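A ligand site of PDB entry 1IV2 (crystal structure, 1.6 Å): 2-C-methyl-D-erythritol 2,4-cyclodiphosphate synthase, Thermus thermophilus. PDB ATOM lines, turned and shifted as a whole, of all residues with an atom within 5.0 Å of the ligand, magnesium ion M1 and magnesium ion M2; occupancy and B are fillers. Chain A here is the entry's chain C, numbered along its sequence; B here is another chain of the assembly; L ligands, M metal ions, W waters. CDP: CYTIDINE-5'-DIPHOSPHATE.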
ATOM      1  N   LEU A 100     -13.202 -22.004  21.547  1.00  0.00           N
ATOM      2  CA  LEU A 100     -14.185 -22.365  20.535  1.00  0.00           C
ATOM      3  C   LEU A 100     -14.886 -23.687  20.832  1.00  0.00           C
ATOM      4  O   LEU A 100     -14.234 -24.681  21.200  1.00  0.00           O
ATOM      5  CB  LEU A 100     -13.545 -22.441  19.143  1.00  0.00           C
ATOM      6  CG  LEU A 100     -12.743 -23.690  18.858  1.00  0.00           C
ATOM      7  CD1 LEU A 100     -12.342 -23.771  17.391  1.00  0.00           C
ATOM      8  CD2 LEU A 100     -11.497 -23.701  19.730  1.00  0.00           C
ATOM      9  N   ASP A 101     -16.198 -23.691  20.668  1.00  0.00           N
ATOM     10  CA  ASP A 101     -17.046 -24.825  21.071  1.00  0.00           C
ATOM     11  C   ASP A 101     -16.821 -25.994  20.108  1.00  0.00           C
ATOM     12  O   ASP A 101     -16.760 -27.146  20.515  1.00  0.00           O
ATOM     13  CB  ASP A 101     -18.517 -24.461  21.119  1.00  0.00           C
ATOM     14  CG  ASP A 101     -18.952 -23.325  22.019  1.00  0.00           C
ATOM     15  OD1 ASP A 101     -18.162 -22.611  22.647  1.00  0.00           O
ATOM     16  OD2 ASP A 101     -20.189 -23.095  22.090  1.00  0.00           O
ATOM     17  N   ARG A 102     -16.704 -25.701  18.822  1.00  0.00           N
ATOM     18  CA  ARG A 102     -16.411 -26.717  17.812  1.00  0.00           C
ATOM     19  C   ARG A 102     -15.638 -26.018  16.713  1.00  0.00           C
ATOM     20  O   ARG A 102     -15.777 -24.817  16.507  1.00  0.00           O
ATOM     21  CB  ARG A 102     -17.664 -27.404  17.263  1.00  0.00           C
ATOM     22  CG  ARG A 102     -18.992 -26.790  17.624  1.00  0.00           C
ATOM     23  CD  ARG A 102     -20.156 -27.412  16.847  1.00  0.00           C
ATOM     24  NE  ARG A 102     -20.884 -26.427  16.069  1.00  0.00           N
ATOM     25  CZ  ARG A 102     -21.628 -26.670  14.997  1.00  0.00           C
ATOM     26  NH1 ARG A 102     -21.778 -27.920  14.546  1.00  0.00           N
ATOM     27  NH2 ARG A 102     -22.251 -25.676  14.366  1.00  0.00           N
ATOM     28  N   PRO A 103     -14.795 -26.745  16.003  1.00  0.00           N
ATOM     29  CA  PRO A 103     -14.597 -28.161  16.226  1.00  0.00           C
ATOM     30  C   PRO A 103     -13.622 -28.453  17.371  1.00  0.00           C
ATOM     31  O   PRO A 103     -12.915 -27.555  17.807  1.00  0.00           O
ATOM     32  CB  PRO A 103     -13.916 -28.589  14.912  1.00  0.00           C
ATOM     33  CG  PRO A 103     -13.191 -27.377  14.438  1.00  0.00           C
ATOM     34  CD  PRO A 103     -13.950 -26.185  14.917  1.00  0.00           C
ATOM     35  N   LYS A 104     -13.576 -29.712  17.800  1.00  0.00           N
ATOM     36  CA  LYS A 104     -12.604 -30.167  18.778  1.00  0.00           C
ATOM     37  C   LYS A 104     -11.195 -30.027  18.220  1.00  0.00           C
ATOM     38  O   LYS A 104     -10.955 -30.449  17.073  1.00  0.00           O
ATOM     39  CB  LYS A 104     -12.839 -31.630  19.165  1.00  0.00           C
ATOM     40  CG  LYS A 104     -14.196 -31.885  19.788  1.00  0.00           C
ATOM     41  CD  LYS A 104     -14.495 -33.360  19.945  1.00  0.00           C
ATOM     42  CE  LYS A 104     -15.169 -33.670  21.279  1.00  0.00           C
ATOM     43  NZ  LYS A 104     -14.192 -34.275  22.239  1.00  0.00           N
ATOM     44  N   LEU A 105     -10.260 -29.491  18.994  1.00  0.00           N
ATOM     45  CA  LEU A 105      -8.914 -29.283  18.453  1.00  0.00           C
ATOM     46  C   LEU A 105      -7.926 -30.323  18.970  1.00  0.00           C
ATOM     47  O   LEU A 105      -6.861 -30.556  18.370  1.00  0.00           O
ATOM     48  CB  LEU A 105      -8.458 -27.831  18.743  1.00  0.00           C
ATOM     49  CG  LEU A 105      -9.216 -26.732  17.975  1.00  0.00           C
ATOM     50  CD1 LEU A 105      -8.521 -25.386  18.167  1.00  0.00           C
ATOM     51  CD2 LEU A 105      -9.352 -27.053  16.499  1.00  0.00           C
ATOM     52  N   GLY A 106      -8.289 -31.006  20.059  1.00  0.00           N
ATOM     53  CA  GLY A 106      -7.487 -32.107  20.568  1.00  0.00           C
ATOM     54  C   GLY A 106      -6.984 -33.075  19.507  1.00  0.00           C
ATOM     55  O   GLY A 106      -5.772 -33.332  19.480  1.00  0.00           O
ATOM     56  N   PRO A 107      -7.792 -33.627  18.631  1.00  0.00           N
ATOM     57  CA  PRO A 107      -7.281 -34.560  17.611  1.00  0.00           C
ATOM     58  C   PRO A 107      -6.223 -33.929  16.720  1.00  0.00           C
ATOM     59  O   PRO A 107      -5.411 -34.622  16.124  1.00  0.00           O
ATOM     60  CB  PRO A 107      -8.514 -34.901  16.765  1.00  0.00           C
ATOM     61  CG  PRO A 107      -9.670 -34.652  17.687  1.00  0.00           C
ATOM     62  CD  PRO A 107      -9.259 -33.457  18.521  1.00  0.00           C
ATOM     63  N   ARG A 109      -3.925 -31.587  17.857  1.00  0.00           N
ATOM     64  CA  ARG A 109      -2.974 -30.902  18.726  1.00  0.00           C
ATOM     65  C   ARG A 109      -1.560 -31.003  18.199  1.00  0.00           C
ATOM     66  O   ARG A 109      -0.875 -29.973  18.193  1.00  0.00           O
ATOM     67  CB  ARG A 109      -3.048 -31.483  20.137  1.00  0.00           C
ATOM     68  CG  ARG A 109      -2.183 -30.853  21.204  1.00  0.00           C
ATOM     69  CD  ARG A 109      -2.368 -31.509  22.575  1.00  0.00           C
ATOM     70  NE  ARG A 109      -3.756 -31.591  22.999  1.00  0.00           N
ATOM     71  CZ  ARG A 109      -4.447 -30.644  23.620  1.00  0.00           C
ATOM     72  NH1 ARG A 109      -3.878 -29.478  23.932  1.00  0.00           N
ATOM     73  NH2 ARG A 109      -5.705 -30.865  23.942  1.00  0.00           N
ATOM     74  N   PHE A 131      -6.623 -25.545  24.722  1.00  0.00           N
ATOM     75  CA  PHE A 131      -7.931 -25.323  24.104  1.00  0.00           C
ATOM     76  C   PHE A 131      -9.055 -25.287  25.129  1.00  0.00           C
ATOM     77  O   PHE A 131      -9.045 -26.073  26.078  1.00  0.00           O
ATOM     78  CB  PHE A 131      -8.323 -26.440  23.125  1.00  0.00           C
ATOM     79  CG  PHE A 131      -7.209 -26.787  22.144  1.00  0.00           C
ATOM     80  CD1 PHE A 131      -6.640 -25.809  21.333  1.00  0.00           C
ATOM     81  CD2 PHE A 131      -6.776 -28.103  22.071  1.00  0.00           C
ATOM     82  CE1 PHE A 131      -5.636 -26.151  20.442  1.00  0.00           C
ATOM     83  CE2 PHE A 131      -5.748 -28.426  21.186  1.00  0.00           C
ATOM     84  CZ  PHE A 131      -5.174 -27.455  20.380  1.00  0.00           C
ATOM     85  N   LYS A 132      -9.997 -24.366  24.912  1.00  0.00           N
ATOM     86  CA  LYS A 132     -11.148 -24.256  25.773  1.00  0.00           C
ATOM     87  C   LYS A 132     -12.430 -24.194  24.947  1.00  0.00           C
ATOM     88  O   LYS A 132     -12.407 -23.627  23.859  1.00  0.00           O
ATOM     89  CB  LYS A 132     -11.082 -22.971  26.607  1.00  0.00           C
ATOM     90  CG  LYS A 132      -9.983 -22.786  27.616  1.00  0.00           C
ATOM     91  CD  LYS A 132      -9.781 -23.982  28.535  1.00  0.00           C
ATOM     92  CE  LYS A 132     -11.068 -24.448  29.188  1.00  0.00           C
ATOM     93  NZ  LYS A 132     -10.798 -25.409  30.294  1.00  0.00           N
ATOM     94  N   THR A 133     -13.549 -24.734  25.457  1.00  0.00           N
ATOM     95  CA  THR A 133     -14.832 -24.355  24.860  1.00  0.00           C
ATOM     96  C   THR A 133     -15.289 -23.016  25.476  1.00  0.00           C
ATOM     97  O   THR A 133     -14.631 -22.555  26.405  1.00  0.00           O
ATOM     98  CB  THR A 133     -15.942 -25.397  25.071  1.00  0.00           C
ATOM     99  OG1 THR A 133     -16.427 -25.314  26.424  1.00  0.00           O
ATOM    100  CG2 THR A 133     -15.439 -26.833  24.883  1.00  0.00           C
ATOM    101  N   GLU A 135     -18.232 -22.601  26.956  1.00  0.00           N
ATOM    102  CA  GLU A 135     -19.204 -23.020  27.968  1.00  0.00           C
ATOM    103  C   GLU A 135     -20.514 -22.266  27.763  1.00  0.00           C
ATOM    104  O   GLU A 135     -21.268 -21.929  28.667  1.00  0.00           O
ATOM    105  CB  GLU A 135     -18.679 -22.835  29.398  1.00  0.00           C
ATOM    106  CG  GLU A 135     -17.372 -23.588  29.684  1.00  0.00           C
ATOM    107  CD  GLU A 135     -17.626 -25.064  29.934  1.00  0.00           C
ATOM    108  OE1 GLU A 135     -16.729 -25.888  29.723  1.00  0.00           O
ATOM    109  OE2 GLU A 135     -18.770 -25.382  30.347  1.00  0.00           O
ATOM    110  N   ASP B   8     -10.105 -20.423  31.719  1.00  0.00           N
ATOM    111  CA  ASP B   8     -11.159 -21.388  32.004  1.00  0.00           C
ATOM    112  C   ASP B   8     -12.441 -20.613  32.273  1.00  0.00           C
ATOM    113  O   ASP B   8     -12.400 -19.476  32.728  1.00  0.00           O
ATOM    114  CB  ASP B   8     -10.860 -22.258  33.229  1.00  0.00           C
ATOM    115  CG  ASP B   8     -11.719 -23.520  33.269  1.00  0.00           C
ATOM    116  OD1 ASP B   8     -12.062 -24.046  32.190  1.00  0.00           O
ATOM    117  OD2 ASP B   8     -12.267 -23.835  34.341  1.00  0.00           O
ATOM    118  N   SER B   9     -13.544 -21.286  31.995  1.00  0.00           N
ATOM    119  CA  SER B   9     -14.807 -20.699  32.374  1.00  0.00           C
ATOM    120  C   SER B   9     -15.802 -21.821  32.679  1.00  0.00           C
ATOM    121  O   SER B   9     -15.647 -22.910  32.146  1.00  0.00           O
ATOM    122  CB  SER B   9     -15.340 -19.765  31.282  1.00  0.00           C
ATOM    123  OG  SER B   9     -15.919 -20.555  30.252  1.00  0.00           O
ATOM    124  N   HIS B  10     -16.781 -21.488  33.534  1.00  0.00           N
ATOM    125  CA  HIS B  10     -17.847 -22.456  33.806  1.00  0.00           C
ATOM    126  C   HIS B  10     -19.153 -21.675  33.891  1.00  0.00           C
ATOM    127  O   HIS B  10     -19.162 -20.544  34.385  1.00  0.00           O
ATOM    128  CB  HIS B  10     -17.584 -23.276  35.077  1.00  0.00           C
ATOM    129  CG  HIS B  10     -16.541 -24.322  34.790  1.00  0.00           C
ATOM    130  ND1 HIS B  10     -16.841 -25.465  34.081  1.00  0.00           N
ATOM    131  CD2 HIS B  10     -15.210 -24.393  35.048  1.00  0.00           C
ATOM    132  CE1 HIS B  10     -15.744 -26.198  33.946  1.00  0.00           C
ATOM    133  NE2 HIS B  10     -14.735 -25.566  34.530  1.00  0.00           N
ATOM    134  N   SER B  35     -16.542 -31.470  36.193  1.00  0.00           N
ATOM    135  CA  SER B  35     -15.536 -31.281  37.237  1.00  0.00           C
ATOM    136  C   SER B  35     -16.138 -30.520  38.416  1.00  0.00           C
ATOM    137  O   SER B  35     -17.358 -30.394  38.503  1.00  0.00           O
ATOM    138  CB  SER B  35     -14.315 -30.503  36.710  1.00  0.00           C
ATOM    139  OG  SER B  35     -14.745 -29.191  36.363  1.00  0.00           O
ATOM    140  N   HIS B  42      -8.373 -24.506  37.269  1.00  0.00           N
ATOM    141  CA  HIS B  42      -8.187 -24.976  35.891  1.00  0.00           C
ATOM    142  C   HIS B  42      -7.253 -24.058  35.103  1.00  0.00           C
ATOM    143  O   HIS B  42      -6.326 -24.506  34.430  1.00  0.00           O
ATOM    144  CB  HIS B  42      -9.543 -25.084  35.191  1.00  0.00           C
ATOM    145  CG  HIS B  42     -10.331 -26.231  35.755  1.00  0.00           C
ATOM    146  ND1 HIS B  42     -11.594 -26.564  35.319  1.00  0.00           N
ATOM    147  CD2 HIS B  42     -10.012 -27.120  36.738  1.00  0.00           C
ATOM    148  CE1 HIS B  42     -12.030 -27.614  36.002  1.00  0.00           C
ATOM    149  NE2 HIS B  42     -11.091 -27.973  36.872  1.00  0.00           N
ATOM    150  N   ASP B  56      -2.963 -29.701  27.774  1.00  0.00           N
ATOM    151  CA  ASP B  56      -3.934 -28.960  28.565  1.00  0.00           C
ATOM    152  C   ASP B  56      -4.663 -29.950  29.452  1.00  0.00           C
ATOM    153  O   ASP B  56      -4.420 -31.159  29.393  1.00  0.00           O
ATOM    154  CB  ASP B  56      -4.856 -28.116  27.694  1.00  0.00           C
ATOM    155  CG  ASP B  56      -5.799 -28.863  26.769  1.00  0.00           C
ATOM    156  OD1 ASP B  56      -6.298 -29.943  27.138  1.00  0.00           O
ATOM    157  OD2 ASP B  56      -6.036 -28.356  25.645  1.00  0.00           O
ATOM    158  N   ILE B  57      -5.561 -29.459  30.295  1.00  0.00           N
ATOM    159  CA  ILE B  57      -6.086 -30.356  31.315  1.00  0.00           C
ATOM    160  C   ILE B  57      -6.990 -31.424  30.709  1.00  0.00           C
ATOM    161  O   ILE B  57      -7.237 -32.450  31.326  1.00  0.00           O
ATOM    162  CB  ILE B  57      -6.894 -29.581  32.392  1.00  0.00           C
ATOM    163  CG1 ILE B  57      -7.984 -28.674  31.823  1.00  0.00           C
ATOM    164  CG2 ILE B  57      -5.926 -28.827  33.262  1.00  0.00           C
ATOM    165  CD1 ILE B  57      -8.971 -28.193  32.874  1.00  0.00           C
ATOM    166  N   GLY B  58      -7.492 -31.113  29.519  1.00  0.00           N
ATOM    167  CA  GLY B  58      -8.367 -32.053  28.811  1.00  0.00           C
ATOM    168  C   GLY B  58      -7.539 -33.211  28.294  1.00  0.00           C
ATOM    169  O   GLY B  58      -8.021 -34.350  28.290  1.00  0.00           O
ATOM    170  N   LEU B  59      -6.311 -32.916  27.889  1.00  0.00           N
ATOM    171  CA  LEU B  59      -5.410 -33.968  27.433  1.00  0.00           C
ATOM    172  C   LEU B  59      -4.896 -34.774  28.624  1.00  0.00           C
ATOM    173  O   LEU B  59      -4.880 -36.016  28.557  1.00  0.00           O
ATOM    174  CB  LEU B  59      -4.221 -33.420  26.654  1.00  0.00           C
ATOM    175  CG  LEU B  59      -3.138 -34.402  26.223  1.00  0.00           C
ATOM    176  CD1 LEU B  59      -3.581 -35.288  25.067  1.00  0.00           C
ATOM    177  CD2 LEU B  59      -1.881 -33.601  25.831  1.00  0.00           C
HETATM  178  O3B CDP L   1     -14.830 -28.054  31.513  1.00  0.00           O
HETATM  179  PB  CDP L   1     -13.374 -27.936  31.154  1.00  0.00           P
HETATM  180  O1B CDP L   1     -12.897 -26.890  32.110  1.00  0.00           O
HETATM  181  O2B CDP L   1     -12.756 -29.327  31.411  1.00  0.00           O
HETATM  182  O3A CDP L   1     -12.980 -27.561  29.743  1.00  0.00           O
HETATM  183  PA  CDP L   1     -13.920 -27.497  28.443  1.00  0.00           P
HETATM  184  O1A CDP L   1     -13.998 -26.045  27.804  1.00  0.00           O
HETATM  185  O2A CDP L   1     -15.107 -28.300  28.395  1.00  0.00           O
HETATM  186  O5' CDP L   1     -12.825 -28.274  27.524  1.00  0.00           O
HETATM  187  C5' CDP L   1     -12.428 -29.570  27.866  1.00  0.00           C
HETATM  188  C4' CDP L   1     -11.383 -29.914  26.914  1.00  0.00           C
HETATM  189  O4' CDP L   1     -11.601 -29.987  25.490  1.00  0.00           O
HETATM  190  C3' CDP L   1     -10.049 -29.124  27.061  1.00  0.00           C
HETATM  191  O3' CDP L   1      -9.366 -29.115  28.332  1.00  0.00           O
HETATM  192  C2' CDP L   1      -9.399 -29.172  25.700  1.00  0.00           C
HETATM  193  O2' CDP L   1      -8.722 -30.384  25.858  1.00  0.00           O
HETATM  194  C1' CDP L   1     -10.343 -29.946  24.837  1.00  0.00           C
HETATM  195  N1  CDP L   1     -10.935 -29.011  23.743  1.00  0.00           N
HETATM  196  C2  CDP L   1     -10.665 -29.289  22.358  1.00  0.00           C
HETATM  197  O2  CDP L   1      -9.938 -30.261  22.040  1.00  0.00           O
HETATM  198  N3  CDP L   1     -11.159 -28.521  21.368  1.00  0.00           N
HETATM  199  C4  CDP L   1     -12.012 -27.402  21.657  1.00  0.00           C
HETATM  200  N4  CDP L   1     -12.529 -26.632  20.673  1.00  0.00           N
HETATM  201  C5  CDP L   1     -12.341 -27.067  23.020  1.00  0.00           C
HETATM  202  C6  CDP L   1     -11.790 -27.875  23.998  1.00  0.00           C
HETATM  203 MG    MG M   1     -12.758 -25.713  33.665  1.00  0.00          MG
HETATM  204 MG    MG M   2     -16.408 -28.232  30.100  1.00  0.00          MG
HETATM  205  O   HOH W   1      -8.050 -26.821  28.562  1.00  0.00           O
HETATM  206  O   HOH W   2      -7.538 -33.083  24.419  1.00  0.00           O
HETATM  207  O   HOH W   3     -16.799 -30.374  30.508  1.00  0.00           O
HETATM  208  O   HOH W   4     -17.911 -28.525  28.653  1.00  0.00           O
HETATM  209  O   HOH W   5     -15.908 -30.140  26.691  1.00  0.00           O
HETATM  210  O   HOH W   6     -14.430 -30.187  24.476  1.00  0.00           O
HETATM  211  O   HOH W   7     -17.899 -28.166  32.080  1.00  0.00           O
HETATM  212  O   HOH W   8     -15.666 -29.815  33.536  1.00  0.00           O
HETATM  213  O   HOH W   9     -10.678 -30.534  30.418  1.00  0.00           O
HETATM  214  O   HOH W  10     -14.075 -23.864  29.516  1.00  0.00           O
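N4 of the ligand sits at hydrogen-bond distance from O of Leu 100 (2.6 Å). The backbone NH (N) of Gly 106 lies within hydrogen-bond range of an oxygen (O2) of the ligand (2.7 Å). N of Leu 105 lies within hydrogen-bond range of N3 of the ligand (2.7 Å). The backbone NH (N) of Thr 133 is in hydrogen-bond range of an oxygen (O1A) of the ligand, 2.7 Å away. OG1 of Thr 133 sits at hydrogen-bond distance from O1A of the ligand, 2.9 Å away. OD1 of Asp 56 of chain B lies within hydrogen-bond range of O2' of the ligand (2.8 Å). The backbone NH (N) of Gly 58 of chain B is in hydrogen-bond range of an oxygen (O3') of the ligand (3.0 Å). The backbone carbonyl oxygen (O) of Pro 103 lies within hydrogen-bond range of a nitrogen (N4) of the ligand, 3.0 Å away. The side-chain amino group of Lys 132 is in hydrogen-bond range of an oxygen (O3A) of the ligand.
The side-chain amino group (NZ) of Lys 132 sits close to the side-chain carboxylate (OD1) of Asp 8 of chain B, 2.7 Å away. The side-chain hydroxyl (OG1) of Thr 133 lies within hydrogen-bond range of the backbone NH (N) of Glu 135, at 3.3 Å. The backbone NH (N) of Leu 100 is in hydrogen-bond range of the backbone carbonyl oxygen (O) of Lys 132 (2.9 Å). OD1 of Asp 56 of chain B sits at hydrogen-bond distance from N of Gly 58 of chain B. OD2 of Asp 56 of chain B sits at hydrogen-bond distance from N of Phe 131 (3.0 Å). The side-chain carboxylate of Asp 56 of chain B is in salt-bridge range of the guanidinium group of Arg 109 (3.0 Å). The backbone NH (N) of Leu 59 of chain B sits at hydrogen-bond distance from the side-chain carboxylate (OD1) of Asp 56 of chain B (3.1 Å).
Lys 104 touches the ligand (CA to N3, 3.4 Å). Arg 109 touches the ligand (NH2 to O2', 3.6 Å). O of Phe 131 touches C2' of the ligand (3.1 Å). CG1 of Ile 57 of chain B touches O3' of the ligand (3.8 Å). Hydrophobic or aromatic side chains that line the ligand: Leu 100, Leu 105, Phe 131, His 10 of chain B and Ile 57 of chain B. Of the 22 residues printed, 16 come within 4 Å of the ligand.
NZ of Lys 132 touches magnesium ion M1, 3.9 Å away. Within 4 Å of magnesium ion M1: Lys 132, Asp 8 of chain B, His 10 of chain B and His 42 of chain B.
One residue has an atom within 4 Å of magnesium ion M2: Glu 135.
Magnesium ion M1 is bound by O1B of the ligand (2.0 Å), OD2 of Asp 8 of chain B (2.1 Å), NE2 of His 10 of chain B (2.2 Å), ND1 of His 42 of chain B (2.2 Å) and OD1 of Asp 8 of chain B (2.3 Å).
Magnesium ion M2 is bound by water W4 (2.1 Å), O3B of the ligand (2.1 Å), O2A of the ligand (2.1 Å), water W3 (2.2 Å), OE1 of Glu 135 (2.4 Å) and water W7 (2.5 Å).
Water W9 bridges an oxygen (O2B) of the ligand (2.6 Å) and the backbone NH (N) of Gly 58 of chain B (3.4 Å). Water W1 bridges an oxygen (O3') of the ligand (2.7 Å) and the backbone carbonyl oxygen (O) of Phe 131 (2.8 Å). Water W10 lies within hydrogen-bond range of an oxygen (O1A) of the ligand, the backbone carbonyl oxygen (O) of Ser 9 of chain B and the backbone carbonyl oxygen (O) of Thr 133. Water W2 bridges the guanidinium group (NH2) of Arg 109 and an oxygen (O2') of the ligand.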
